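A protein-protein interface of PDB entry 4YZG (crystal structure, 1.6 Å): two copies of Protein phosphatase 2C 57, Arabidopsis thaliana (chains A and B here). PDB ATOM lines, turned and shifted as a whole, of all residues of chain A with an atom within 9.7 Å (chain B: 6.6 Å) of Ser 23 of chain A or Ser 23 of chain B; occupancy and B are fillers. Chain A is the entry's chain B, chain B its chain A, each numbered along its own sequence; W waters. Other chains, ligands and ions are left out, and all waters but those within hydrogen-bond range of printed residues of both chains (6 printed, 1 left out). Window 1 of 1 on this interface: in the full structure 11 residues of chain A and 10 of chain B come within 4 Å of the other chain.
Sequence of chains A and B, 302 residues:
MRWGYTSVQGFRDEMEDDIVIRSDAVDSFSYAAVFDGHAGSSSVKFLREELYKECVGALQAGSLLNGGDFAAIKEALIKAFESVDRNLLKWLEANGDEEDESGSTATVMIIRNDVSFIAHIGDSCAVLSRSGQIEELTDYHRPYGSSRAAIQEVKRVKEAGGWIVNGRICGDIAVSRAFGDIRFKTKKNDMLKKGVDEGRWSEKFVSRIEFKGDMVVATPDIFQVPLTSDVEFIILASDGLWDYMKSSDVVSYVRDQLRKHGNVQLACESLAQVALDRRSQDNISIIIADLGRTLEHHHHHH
The backbone NH (N) of Ala 25 of chain A sits at hydrogen-bond distance from the backbone carbonyl oxygen (O) of Ile 21 of chain B (3.1 Å).
The side-chain carboxylate (OD2) of Asp 24 of chain A lies within salt-bridge range of the guanidinium group (NE) of Arg 22 of chain B.
The backbone carbonyl oxygen (O) of Ser 23 of chain B sits at hydrogen-bond distance from the backbone NH (N) of Ser 23 of chain A (2.9 Å).
NE of Arg 22 of chain A is in salt-bridge range of OD2 of Asp 24 of chain B, at 2.9 Å.
The backbone NH (N) of Ala 25 of chain B lies within hydrogen-bond range of the backbone carbonyl oxygen (O) of Ile 21 of chain A (2.9 Å).
O of Arg 22 of chain B sits at hydrogen-bond distance from N of Tyr 31 of chain B.
The backbone NH (N) of Asp 24 of chain B is in hydrogen-bond range of the backbone carbonyl oxygen (O) of Phe 29 of chain B (2.8 Å).
The backbone NH (N) of Arg 22 of chain A is in hydrogen-bond range of the backbone carbonyl oxygen (O) of Tyr 31 of chain A.
The side-chain carboxylate (OD1) of Asp 24 of chain A lies within hydrogen-bond range of the backbone NH (N) of Val 26 of chain A, 3.1 Å away.
The backbone NH of Asp 27 of chain A lies within hydrogen-bond range of the side-chain carboxylate of Asp 24 of chain A, 3.0 Å away.
O of Ile 21 of chain A touches CA of Asp 24 of chain B, 3.4 Å away.
O of Ser 23 of chain B touches CA of Arg 22 of chain A (3.2 Å).
O of Ser 23 of chain A touches O of Ile 21 of chain B (3.96 Å).
Ser 23 of chain A touches Arg 22 of chain B (O to CA, 3.3 Å).
O of Ile 21 of chain B touches CA of Asp 24 of chain A, 3.4 Å away.
CG2 of Val 26 of chain A touches N of Ile 21 of chain B, 3.7 Å away.
Arg 2 of chain A touches none of the printed residues of chain B.
Of chain B, only Ile 21, Arg 22 and Ser 23 come within 4 Å of Ser 23 of chain A.
Of the printed residues of chain B, Ala 25 of chain A touches Ile 21.
Of chain A, only Arg 22 (3.2 Å) and Ser 23 (2.9 Å) come within 4 Å of Ser 23 of chain B.
Printed residues of chain A within 4 Å of Ala 25 of chain B: Ile 21 (2.9 Å).
The nearest residue of chain B that does not touch Ser 23 of chain A is Asp 24 of chain B (4.9 Å).
The nearest residue of chain A that does not touch Ser 23 of chain B is Ile 21 of chain A (4.1 Å).
The nearest printed residue of chain B that does not touch Ala 25 of chain A is Trp 3 of chain B (4.4 Å).
Hydrophobic or aromatic side chains of chain A that line the printed part of chain B: Ile 21, Ala 25 and Val 26.
Among the printed residues, 11 pairs touch across the chains.
Ile 21 of chain A touches Ala 25 of chain B, and with the chains exchanged Ala 25 of chain A touches Ile 21 of chain B.
Arg 22 of chain A touches Ser 23 of chain B, and with the chains exchanged Ser 23 of chain A touches Arg 22 of chain B.
Ser 23 of chain A touches Ile 21 of chain B, but with the chains exchanged Ile 21 of chain A does not touch Ser 23 of chain B (4.1 Å).
Ser 23 of chain A touches its own counterpart, Ser 23 of chain B.
Positions printed for both chains: 1, 3, 21, 22, 23, 24, 25, 29, 30, 31 and 52.
Water W5 lies within hydrogen-bond range of the side-chain carboxylate of Asp 24 of chain B (2.6 Å), the backbone NH of Ile 21 of chain A (3.0 Å) and the guanidinium group of Arg 22 of chain A (3.2 Å).
Water W4 lies within hydrogen-bond range of OD1 of Asp 24 of chain A (2.7 Å), N of Ile 21 of chain B (2.9 Å) and NE of Arg 22 of chain B (3.1 Å).
Water W1 lies within hydrogen-bond range of OH of Tyr 52 of chain A (2.8 Å), OD2 of Asp 24 of chain A (2.9 Å) and NE of Arg 22 of chain B (3.4 Å).
Water W3 bridges the side-chain hydroxyl of Ser 23 of chain B and the backbone NH of Ala 25 of chain A.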
ATOM      1  N   MET A   1     -32.553  18.246 -18.754  1.00  0.00           N
ATOM      2  CA  MET A   1     -33.790  18.985 -18.910  1.00  0.00           C
ATOM      3  C   MET A   1     -33.585  20.476 -19.060  1.00  0.00           C
ATOM      4  O   MET A   1     -32.547  20.988 -18.781  1.00  0.00           O
ATOM      5  CB  MET A   1     -34.721  18.707 -17.761  1.00  0.00           C
ATOM      6  CG  MET A   1     -34.165  19.010 -16.413  1.00  0.00           C
ATOM      7  SD  MET A   1     -34.770  20.554 -15.754  1.00  0.00           S
ATOM      8  CE  MET A   1     -33.716  20.526 -14.349  1.00  0.00           C
ATOM      9  N   ARG A   2     -34.606  21.145 -19.538  1.00  0.00           N
ATOM     10  CA  ARG A   2     -34.524  22.573 -19.809  1.00  0.00           C
ATOM     11  C   ARG A   2     -35.666  23.274 -19.107  1.00  0.00           C
ATOM     12  O   ARG A   2     -36.737  22.701 -18.951  1.00  0.00           O
ATOM     13  CB  ARG A   2     -34.595  22.841 -21.311  1.00  0.00           C
ATOM     14  CG  ARG A   2     -33.369  22.374 -22.072  1.00  0.00           C
ATOM     15  CD  ARG A   2     -33.533  22.551 -23.569  1.00  0.00           C
ATOM     16  NE  ARG A   2     -32.236  22.524 -24.244  1.00  0.00           N
ATOM     17  CZ  ARG A   2     -32.056  22.212 -25.523  1.00  0.00           C
ATOM     18  NH1 ARG A   2     -33.092  21.886 -26.286  1.00  0.00           N
ATOM     19  NH2 ARG A   2     -30.833  22.219 -26.040  1.00  0.00           N
ATOM     20  N   TRP A   3     -35.436  24.522 -18.697  1.00  0.00           N
ATOM     21  CA  TRP A   3     -36.460  25.306 -18.016  1.00  0.00           C
ATOM     22  C   TRP A   3     -37.111  26.356 -18.909  1.00  0.00           C
ATOM     23  O   TRP A   3     -36.448  27.019 -19.713  1.00  0.00           O
ATOM     24  CB  TRP A   3     -35.867  26.040 -16.813  1.00  0.00           C
ATOM     25  CG  TRP A   3     -35.325  25.180 -15.726  1.00  0.00           C
ATOM     26  CD1 TRP A   3     -34.012  24.935 -15.457  1.00  0.00           C
ATOM     27  CD2 TRP A   3     -36.077  24.470 -14.734  1.00  0.00           C
ATOM     28  NE1 TRP A   3     -33.898  24.116 -14.360  1.00  0.00           N
ATOM     29  CE2 TRP A   3     -35.150  23.814 -13.900  1.00  0.00           C
ATOM     30  CE3 TRP A   3     -37.446  24.331 -14.463  1.00  0.00           C
ATOM     31  CZ2 TRP A   3     -35.544  23.025 -12.817  1.00  0.00           C
ATOM     32  CZ3 TRP A   3     -37.834  23.554 -13.387  1.00  0.00           C
ATOM     33  CH2 TRP A   3     -36.888  22.906 -12.579  1.00  0.00           C
ATOM     34  N   VAL A  20     -38.593  31.237  -8.471  1.00  0.00           N
ATOM     35  CA  VAL A  20     -37.182  31.003  -8.191  1.00  0.00           C
ATOM     36  C   VAL A  20     -36.780  29.733  -8.914  1.00  0.00           C
ATOM     37  O   VAL A  20     -37.494  28.735  -8.847  1.00  0.00           O
ATOM     38  CB  VAL A  20     -36.934  30.800  -6.673  1.00  0.00           C
ATOM     39  CG1 VAL A  20     -35.501  30.357  -6.414  1.00  0.00           C
ATOM     40  CG2 VAL A  20     -37.251  32.084  -5.905  1.00  0.00           C
ATOM     41  N   ILE A  21     -35.669  29.770  -9.640  1.00  0.00           N
ATOM     42  CA  ILE A  21     -35.111  28.561 -10.210  1.00  0.00           C
ATOM     43  C   ILE A  21     -33.604  28.614  -9.965  1.00  0.00           C
ATOM     44  O   ILE A  21     -32.925  29.491 -10.498  1.00  0.00           O
ATOM     45  CB  ILE A  21     -35.376  28.447 -11.715  1.00  0.00           C
ATOM     46  CG1 ILE A  21     -36.880  28.389 -11.996  1.00  0.00           C
ATOM     47  CG2 ILE A  21     -34.691  27.205 -12.265  1.00  0.00           C
ATOM     48  CD1 ILE A  21     -37.186  28.407 -13.498  1.00  0.00           C
ATOM     49  N   ARG A  22     -33.127  27.674  -9.174  1.00  0.00           N
ATOM     50  CA  ARG A  22     -31.727  27.780  -8.725  1.00  0.00           C
ATOM     51  C   ARG A  22     -31.037  26.455  -8.909  1.00  0.00           C
ATOM     52  O   ARG A  22     -31.631  25.408  -8.698  1.00  0.00           O
ATOM     53  CB  ARG A  22     -31.646  28.087  -7.232  1.00  0.00           C
ATOM     54  CG  ARG A  22     -32.249  29.372  -6.796  1.00  0.00           C
ATOM     55  CD  ARG A  22     -31.501  30.565  -7.289  1.00  0.00           C
ATOM     56  NE  ARG A  22     -32.150  31.790  -6.821  1.00  0.00           N
ATOM     57  CZ  ARG A  22     -31.932  32.353  -5.637  1.00  0.00           C
ATOM     58  NH1 ARG A  22     -31.070  31.799  -4.788  1.00  0.00           N
ATOM     59  NH2 ARG A  22     -32.580  33.467  -5.304  1.00  0.00           N
ATOM     60  N   SER A  23     -29.879  26.198  -9.288  1.00  0.00           N
ATOM     61  CA  SER A  23     -29.313  24.883  -9.490  1.00  0.00           C
ATOM     62  C   SER A  23     -27.975  24.806  -8.791  1.00  0.00           C
ATOM     63  O   SER A  23     -27.279  25.822  -8.621  1.00  0.00           O
ATOM     64  CB  SER A  23     -29.141  24.607 -10.979  1.00  0.00           C
ATOM     65  OG  SER A  23     -30.414  24.598 -11.619  1.00  0.00           O
ATOM     66  N   ASP A  24     -27.630  23.597  -8.365  1.00  0.00           N
ATOM     67  CA  ASP A  24     -26.303  23.315  -7.823  1.00  0.00           C
ATOM     68  C   ASP A  24     -25.725  22.248  -8.731  1.00  0.00           C
ATOM     69  O   ASP A  24     -26.145  21.100  -8.700  1.00  0.00           O
ATOM     70  CB  ASP A  24     -26.445  22.802  -6.399  1.00  0.00           C
ATOM     71  CG  ASP A  24     -25.121  22.593  -5.711  1.00  0.00           C
ATOM     72  OD1 ASP A  24     -24.139  22.162  -6.369  1.00  0.00           O
ATOM     73  OD2 ASP A  24     -25.067  22.860  -4.494  1.00  0.00           O
ATOM     74  N   ALA A  25     -24.777  22.628  -9.579  1.00  0.00           N
ATOM     75  CA  ALA A  25     -24.274  21.695 -10.561  1.00  0.00           C
ATOM     76  C   ALA A  25     -23.445  20.598  -9.907  1.00  0.00           C
ATOM     77  O   ALA A  25     -23.447  19.459 -10.369  1.00  0.00           O
ATOM     78  CB  ALA A  25     -23.439  22.427 -11.607  1.00  0.00           C
ATOM     79  N   VAL A  26     -22.718  20.940  -8.850  1.00  0.00           N
ATOM     80  CA  VAL A  26     -21.824  19.968  -8.222  1.00  0.00           C
ATOM     81  C   VAL A  26     -22.627  18.871  -7.538  1.00  0.00           C
ATOM     82  O   VAL A  26     -22.283  17.700  -7.630  1.00  0.00           O
ATOM     83  CB  VAL A  26     -20.860  20.636  -7.225  1.00  0.00           C
ATOM     84  CG1 VAL A  26     -20.008  19.582  -6.504  1.00  0.00           C
ATOM     85  CG2 VAL A  26     -19.963  21.625  -7.968  1.00  0.00           C
ATOM     86  N   ASP A  27     -23.720  19.260  -6.889  1.00  0.00           N
ATOM     87  CA  ASP A  27     -24.588  18.290  -6.214  1.00  0.00           C
ATOM     88  C   ASP A  27     -25.751  17.797  -7.081  1.00  0.00           C
ATOM     89  O   ASP A  27     -26.636  17.068  -6.605  1.00  0.00           O
ATOM     90  CB  ASP A  27     -25.088  18.863  -4.892  1.00  0.00           C
ATOM     91  CG  ASP A  27     -23.972  18.991  -3.862  1.00  0.00           C
ATOM     92  OD1 ASP A  27     -22.936  18.302  -4.006  1.00  0.00           O
ATOM     93  OD2 ASP A  27     -24.127  19.786  -2.912  1.00  0.00           O
ATOM     94  N   SER A  28     -25.738  18.191  -8.354  1.00  0.00           N
ATOM     95  CA  SER A  28     -26.713  17.720  -9.337  1.00  0.00           C
ATOM     96  C   SER A  28     -28.149  17.894  -8.893  1.00  0.00           C
ATOM     97  O   SER A  28     -28.970  16.979  -9.006  1.00  0.00           O
ATOM     98  CB  SER A  28     -26.461  16.252  -9.671  1.00  0.00           C
ATOM     99  OG  SER A  28     -25.164  16.082 -10.200  1.00  0.00           O
ATOM    100  N   PHE A  29     -28.491  19.059  -8.389  1.00  0.00           N
ATOM    101  CA  PHE A  29     -29.892  19.262  -8.127  1.00  0.00           C
ATOM    102  C   PHE A  29     -30.347  20.640  -8.535  1.00  0.00           C
ATOM    103  O   PHE A  29     -29.554  21.555  -8.732  1.00  0.00           O
ATOM    104  CB  PHE A  29     -30.268  18.932  -6.677  1.00  0.00           C
ATOM    105  CG  PHE A  29     -29.866  19.983  -5.692  1.00  0.00           C
ATOM    106  CD1 PHE A  29     -30.666  21.095  -5.479  1.00  0.00           C
ATOM    107  CD2 PHE A  29     -28.701  19.848  -4.964  1.00  0.00           C
ATOM    108  CE1 PHE A  29     -30.298  22.069  -4.587  1.00  0.00           C
ATOM    109  CE2 PHE A  29     -28.334  20.812  -4.053  1.00  0.00           C
ATOM    110  CZ  PHE A  29     -29.131  21.924  -3.867  1.00  0.00           C
ATOM    111  N   SER A  30     -31.651  20.767  -8.682  1.00  0.00           N
ATOM    112  CA  SER A  30     -32.247  22.056  -8.949  1.00  0.00           C
ATOM    113  C   SER A  30     -33.410  22.256  -8.011  1.00  0.00           C
ATOM    114  O   SER A  30     -33.990  21.297  -7.493  1.00  0.00           O
ATOM    115  CB  SER A  30     -32.746  22.130 -10.385  1.00  0.00           C
ATOM    116  OG  SER A  30     -33.600  21.040 -10.665  1.00  0.00           O
ATOM    117  N   TYR A  31     -33.736  23.522  -7.830  1.00  0.00           N
ATOM    118  CA  TYR A  31     -34.841  23.952  -6.971  1.00  0.00           C
ATOM    119  C   TYR A  31     -35.660  24.927  -7.785  1.00  0.00           C
ATOM    120  O   TYR A  31     -35.115  25.909  -8.308  1.00  0.00           O
ATOM    121  CB  TYR A  31     -34.265  24.626  -5.723  1.00  0.00           C
ATOM    122  CG  TYR A  31     -35.188  25.422  -4.807  1.00  0.00           C
ATOM    123  CD1 TYR A  31     -35.541  26.735  -5.109  1.00  0.00           C
ATOM    124  CD2 TYR A  31     -35.592  24.908  -3.585  1.00  0.00           C
ATOM    125  CE1 TYR A  31     -36.353  27.490  -4.246  1.00  0.00           C
ATOM    126  CE2 TYR A  31     -36.406  25.653  -2.717  1.00  0.00           C
ATOM    127  CZ  TYR A  31     -36.768  26.936  -3.043  1.00  0.00           C
ATOM    128  OH  TYR A  31     -37.555  27.708  -2.199  1.00  0.00           O
ATOM    129  N   ALA A  32     -36.963  24.671  -7.879  1.00  0.00           N
ATOM    130  CA  ALA A  32     -37.867  25.589  -8.560  1.00  0.00           C
ATOM    131  C   ALA A  32     -39.007  25.914  -7.635  1.00  0.00           C
ATOM    132  O   ALA A  32     -39.532  25.023  -6.963  1.00  0.00           O
ATOM    133  CB  ALA A  32     -38.405  24.970  -9.830  1.00  0.00           C
ATOM    134  N   TYR A  52     -34.976  28.619  -0.039  1.00  0.00           N
ATOM    135  CA  TYR A  52     -33.945  27.796  -0.698  1.00  0.00           C
ATOM    136  C   TYR A  52     -32.858  27.369   0.259  1.00  0.00           C
ATOM    137  O   TYR A  52     -32.543  26.264   0.346  1.00  0.00           O
ATOM    138  CB  TYR A  52     -33.322  28.511  -1.906  1.00  0.00           C
ATOM    139  CG  TYR A  52     -32.163  27.780  -2.565  1.00  0.00           C
ATOM    140  CD1 TYR A  52     -30.879  27.899  -2.098  1.00  0.00           C
ATOM    141  CD2 TYR A  52     -32.340  27.003  -3.634  1.00  0.00           C
ATOM    142  CE1 TYR A  52     -29.837  27.228  -2.688  1.00  0.00           C
ATOM    143  CE2 TYR A  52     -31.302  26.360  -4.250  1.00  0.00           C
ATOM    144  CZ  TYR A  52     -30.045  26.463  -3.775  1.00  0.00           C
ATOM    145  OH  TYR A  52     -29.044  25.778  -4.414  1.00  0.00           O
ATOM    146  N   VAL A  56     -32.199  23.409   1.178  1.00  0.00           N
ATOM    147  CA  VAL A  56     -30.961  22.808   0.731  1.00  0.00           C
ATOM    148  C   VAL A  56     -30.079  22.444   1.910  1.00  0.00           C
ATOM    149  O   VAL A  56     -29.454  21.383   1.921  1.00  0.00           O
ATOM    150  CB  VAL A  56     -30.231  23.717  -0.260  1.00  0.00           C
ATOM    151  CG1 VAL A  56     -28.893  23.115  -0.647  1.00  0.00           C
ATOM    152  CG2 VAL A  56     -31.132  23.916  -1.475  1.00  0.00           C
ATOM    153  N   GLN A  60     -28.836  18.686   2.642  1.00  0.00           N
ATOM    154  CA  GLN A  60     -27.440  18.413   2.607  1.00  0.00           C
ATOM    155  C   GLN A  60     -26.971  17.894   3.943  1.00  0.00           C
ATOM    156  O   GLN A  60     -25.915  17.267   4.020  1.00  0.00           O
ATOM    157  CB  GLN A  60     -26.660  19.631   2.160  1.00  0.00           C
ATOM    158  CG  GLN A  60     -26.817  19.844   0.674  1.00  0.00           C
ATOM    159  CD  GLN A  60     -26.070  21.066   0.256  1.00  0.00           C
ATOM    160  OE1 GLN A  60     -25.792  21.970   1.049  1.00  0.00           O
ATOM    161  NE2 GLN A  60     -25.736  21.111  -1.031  1.00  0.00           N
ATOM    162  N   MET A 109     -40.327  22.524  -6.160  1.00  0.00           N
ATOM    163  CA  MET A 109     -39.870  21.250  -6.686  1.00  0.00           C
ATOM    164  C   MET A 109     -38.359  21.168  -6.582  1.00  0.00           C
ATOM    165  O   MET A 109     -37.640  22.087  -6.980  1.00  0.00           O
ATOM    166  CB  MET A 109     -40.271  21.074  -8.145  1.00  0.00           C
ATOM    167  CG  MET A 109     -39.735  19.797  -8.742  1.00  0.00           C
ATOM    168  SD  MET A 109     -40.502  19.437 -10.338  1.00  0.00           S
ATOM    169  CE  MET A 109     -39.770  20.705 -11.370  1.00  0.00           C
ATOM    170  N   ILE A 110     -37.883  20.067  -6.030  1.00  0.00           N
ATOM    171  CA  ILE A 110     -36.450  19.775  -6.033  1.00  0.00           C
ATOM    172  C   ILE A 110     -36.242  18.582  -6.928  1.00  0.00           C
ATOM    173  O   ILE A 110     -36.897  17.562  -6.757  1.00  0.00           O
ATOM    174  CB  ILE A 110     -35.957  19.524  -4.603  1.00  0.00           C
ATOM    175  CG1 ILE A 110     -36.131  20.832  -3.812  1.00  0.00           C
ATOM    176  CG2 ILE A 110     -34.508  19.044  -4.581  1.00  0.00           C
ATOM    177  CD1 ILE A 110     -35.807  20.751  -2.367  1.00  0.00           C
ATOM    178  N   ILE A 111     -35.353  18.715  -7.901  1.00  0.00           N
ATOM    179  CA  ILE A 111     -35.032  17.599  -8.793  1.00  0.00           C
ATOM    180  C   ILE A 111     -33.576  17.148  -8.664  1.00  0.00           C
ATOM    181  O   ILE A 111     -32.701  17.955  -8.687  1.00  0.00           O
ATOM    182  CB  ILE A 111     -35.159  17.937 -10.252  1.00  0.00           C
ATOM    183  CG1 ILE A 111     -36.584  18.236 -10.637  1.00  0.00           C
ATOM    184  CG2 ILE A 111     -34.650  16.746 -11.053  1.00  0.00           C
ATOM    185  CD1 ILE A 111     -36.798  18.483 -12.092  1.00  0.00           C
ATOM    186  N   MET B   1     -25.369  27.624 -21.723  1.00  0.00           N
ATOM    187  CA  MET B   1     -24.060  27.171 -21.298  1.00  0.00           C
ATOM    188  C   MET B   1     -24.170  25.855 -20.545  1.00  0.00           C
ATOM    189  O   MET B   1     -25.232  25.518 -20.015  1.00  0.00           O
ATOM    190  CB  MET B   1     -23.409  28.210 -20.402  1.00  0.00           C
ATOM    191  CG  MET B   1     -23.719  28.014 -18.942  1.00  0.00           C
ATOM    192  SD  MET B   1     -22.222  28.215 -17.983  1.00  0.00           S
ATOM    193  CE  MET B   1     -21.846  29.887 -18.435  1.00  0.00           C
ATOM    194  N   TRP B   3     -21.908  23.119 -17.800  1.00  0.00           N
ATOM    195  CA  TRP B   3     -20.803  22.997 -16.860  1.00  0.00           C
ATOM    196  C   TRP B   3     -20.167  21.622 -16.879  1.00  0.00           C
ATOM    197  O   TRP B   3     -20.877  20.607 -16.930  1.00  0.00           O
ATOM    198  CB  TRP B   3     -21.265  23.254 -15.425  1.00  0.00           C
ATOM    199  CG  TRP B   3     -21.789  24.622 -15.172  1.00  0.00           C
ATOM    200  CD1 TRP B   3     -23.093  24.996 -15.137  1.00  0.00           C
ATOM    201  CD2 TRP B   3     -21.024  25.799 -14.897  1.00  0.00           C
ATOM    202  NE1 TRP B   3     -23.193  26.338 -14.868  1.00  0.00           N
ATOM    203  CE2 TRP B   3     -21.937  26.852 -14.708  1.00  0.00           C
ATOM    204  CE3 TRP B   3     -19.658  26.069 -14.804  1.00  0.00           C
ATOM    205  CZ2 TRP B   3     -21.526  28.156 -14.427  1.00  0.00           C
ATOM    206  CZ3 TRP B   3     -19.251  27.358 -14.520  1.00  0.00           C
ATOM    207  CH2 TRP B   3     -20.182  28.387 -14.342  1.00  0.00           C
ATOM    208  N   ILE B  21     -20.585  25.306  -7.653  1.00  0.00           N
ATOM    209  CA  ILE B  21     -21.191  25.881  -8.868  1.00  0.00           C
ATOM    210  C   ILE B  21     -22.678  26.051  -8.588  1.00  0.00           C
ATOM    211  O   ILE B  21     -23.395  25.066  -8.373  1.00  0.00           O
ATOM    212  CB  ILE B  21     -21.039  24.960 -10.108  1.00  0.00           C
ATOM    213  CG1 ILE B  21     -19.571  24.656 -10.400  1.00  0.00           C
ATOM    214  CG2 ILE B  21     -21.654  25.630 -11.351  1.00  0.00           C
ATOM    215  CD1 ILE B  21     -19.412  23.644 -11.557  1.00  0.00           C
ATOM    216  N   ARG B  22     -23.146  27.300  -8.549  1.00  0.00           N
ATOM    217  CA  ARG B  22     -24.546  27.602  -8.223  1.00  0.00           C
ATOM    218  C   ARG B  22     -25.084  28.532  -9.287  1.00  0.00           C
ATOM    219  O   ARG B  22     -24.444  29.514  -9.632  1.00  0.00           O
ATOM    220  CB  ARG B  22     -24.645  28.316  -6.875  1.00  0.00           C
ATOM    221  CG  ARG B  22     -23.888  27.681  -5.736  1.00  0.00           C
ATOM    222  CD  ARG B  22     -24.577  26.479  -5.213  1.00  0.00           C
ATOM    223  NE  ARG B  22     -23.758  25.765  -4.220  1.00  0.00           N
ATOM    224  CZ  ARG B  22     -23.676  26.024  -2.916  1.00  0.00           C
ATOM    225  NH1 ARG B  22     -24.362  27.023  -2.343  1.00  0.00           N
ATOM    226  NH2 ARG B  22     -22.871  25.267  -2.174  1.00  0.00           N
ATOM    227  N   SER B  23     -26.233  28.194  -9.853  1.00  0.00           N
ATOM    228  CA  SER B  23     -26.820  28.992 -10.921  1.00  0.00           C
ATOM    229  C   SER B  23     -28.218  29.475 -10.543  1.00  0.00           C
ATOM    230  O   SER B  23     -28.907  28.837  -9.770  1.00  0.00           O
ATOM    231  CB  SER B  23     -26.901  28.160 -12.195  1.00  0.00           C
ATOM    232  OG  SER B  23     -25.587  27.873 -12.662  1.00  0.00           O
ATOM    233  N   ASP B  24     -28.611  30.621 -11.087  1.00  0.00           N
ATOM    234  CA  ASP B  24     -29.944  31.169 -10.858  1.00  0.00           C
ATOM    235  C   ASP B  24     -30.474  31.464 -12.244  1.00  0.00           C
ATOM    236  O   ASP B  24     -30.014  32.399 -12.892  1.00  0.00           O
ATOM    237  CB  ASP B  24     -29.837  32.463 -10.046  1.00  0.00           C
ATOM    238  CG  ASP B  24     -31.183  33.120  -9.770  1.00  0.00           C
ATOM    239  OD1 ASP B  24     -32.116  33.014 -10.587  1.00  0.00           O
ATOM    240  OD2 ASP B  24     -31.301  33.778  -8.722  1.00  0.00           O
ATOM    241  N   ALA B  25     -31.424  30.662 -12.708  1.00  0.00           N
ATOM    242  CA  ALA B  25     -31.921  30.786 -14.080  1.00  0.00           C
ATOM    243  C   ALA B  25     -32.712  32.062 -14.308  1.00  0.00           C
ATOM    244  O   ALA B  25     -32.603  32.710 -15.365  1.00  0.00           O
ATOM    245  CB  ALA B  25     -32.778  29.574 -14.441  1.00  0.00           C
ATOM    246  N   PHE B  29     -27.748  34.364 -13.577  1.00  0.00           N
ATOM    247  CA  PHE B  29     -26.609  34.605 -12.707  1.00  0.00           C
ATOM    248  C   PHE B  29     -25.989  33.269 -12.377  1.00  0.00           C
ATOM    249  O   PHE B  29     -26.691  32.293 -12.160  1.00  0.00           O
ATOM    250  CB  PHE B  29     -27.114  35.250 -11.405  1.00  0.00           C
ATOM    251  CG  PHE B  29     -26.070  35.402 -10.333  1.00  0.00           C
ATOM    252  CD1 PHE B  29     -25.853  34.394  -9.397  1.00  0.00           C
ATOM    253  CD2 PHE B  29     -25.345  36.580 -10.220  1.00  0.00           C
ATOM    254  CE1 PHE B  29     -24.899  34.539  -8.403  1.00  0.00           C
ATOM    255  CE2 PHE B  29     -24.388  36.729  -9.215  1.00  0.00           C
ATOM    256  CZ  PHE B  29     -24.166  35.714  -8.314  1.00  0.00           C
ATOM    257  N   SER B  30     -24.670  33.206 -12.322  1.00  0.00           N
ATOM    258  CA  SER B  30     -24.078  32.008 -11.745  1.00  0.00           C
ATOM    259  C   SER B  30     -22.822  32.353 -10.980  1.00  0.00           C
ATOM    260  O   SER B  30     -22.197  33.384 -11.217  1.00  0.00           O
ATOM    261  CB  SER B  30     -23.757  30.985 -12.830  1.00  0.00           C
ATOM    262  OG  SER B  30     -22.830  31.533 -13.743  1.00  0.00           O
ATOM    263  N   TYR B  31     -22.475  31.460 -10.055  1.00  0.00           N
ATOM    264  CA  TYR B  31     -21.284  31.599  -9.220  1.00  0.00           C
ATOM    265  C   TYR B  31     -20.542  30.272  -9.268  1.00  0.00           C
ATOM    266  O   TYR B  31     -21.139  29.230  -8.988  1.00  0.00           O
ATOM    267  CB  TYR B  31     -21.741  31.907  -7.796  1.00  0.00           C
ATOM    268  CG  TYR B  31     -20.687  31.850  -6.697  1.00  0.00           C
ATOM    269  CD1 TYR B  31     -20.314  30.634  -6.128  1.00  0.00           C
ATOM    270  CD2 TYR B  31     -20.118  33.025  -6.181  1.00  0.00           C
ATOM    271  CE1 TYR B  31     -19.378  30.586  -5.102  1.00  0.00           C
ATOM    272  CE2 TYR B  31     -19.162  32.970  -5.153  1.00  0.00           C
ATOM    273  CZ  TYR B  31     -18.815  31.746  -4.618  1.00  0.00           C
ATOM    274  OH  TYR B  31     -17.902  31.653  -3.567  1.00  0.00           O
ATOM    275  N   TYR B  52     -20.039  32.528  -1.062  1.00  0.00           N
ATOM    276  CA  TYR B  52     -21.193  32.613  -1.951  1.00  0.00           C
ATOM    277  C   TYR B  52     -22.203  33.573  -1.366  1.00  0.00           C
ATOM    278  O   TYR B  52     -22.623  34.487  -2.000  1.00  0.00           O
ATOM    279  CB  TYR B  52     -21.804  31.247  -2.152  1.00  0.00           C
ATOM    280  CG  TYR B  52     -23.126  31.253  -2.821  1.00  0.00           C
ATOM    281  CD1 TYR B  52     -23.256  31.515  -4.160  1.00  0.00           C
ATOM    282  CD2 TYR B  52     -24.248  30.986  -2.098  1.00  0.00           C
ATOM    283  CE1 TYR B  52     -24.463  31.518  -4.780  1.00  0.00           C
ATOM    284  CE2 TYR B  52     -25.478  31.013  -2.691  1.00  0.00           C
ATOM    285  CZ  TYR B  52     -25.581  31.272  -4.023  1.00  0.00           C
ATOM    286  OH  TYR B  52     -26.824  31.278  -4.585  1.00  0.00           O
HETATM  287  O   HOH W   1     -26.812  24.685  -3.150  1.00  0.00           O
HETATM  288  O   HOH W   2     -25.829  24.993  -0.451  1.00  0.00           O
HETATM  289  O   HOH W   3     -25.499  25.244 -11.579  1.00  0.00           O
HETATM  290  O   HOH W   4     -21.947  23.676  -5.692  1.00  0.00           O
HETATM  291  O   HOH W   5     -34.256  32.355  -9.181  1.00  0.00           O
HETATM  292  O   HOH W   6     -30.581  27.271 -12.542  1.00  0.00           O
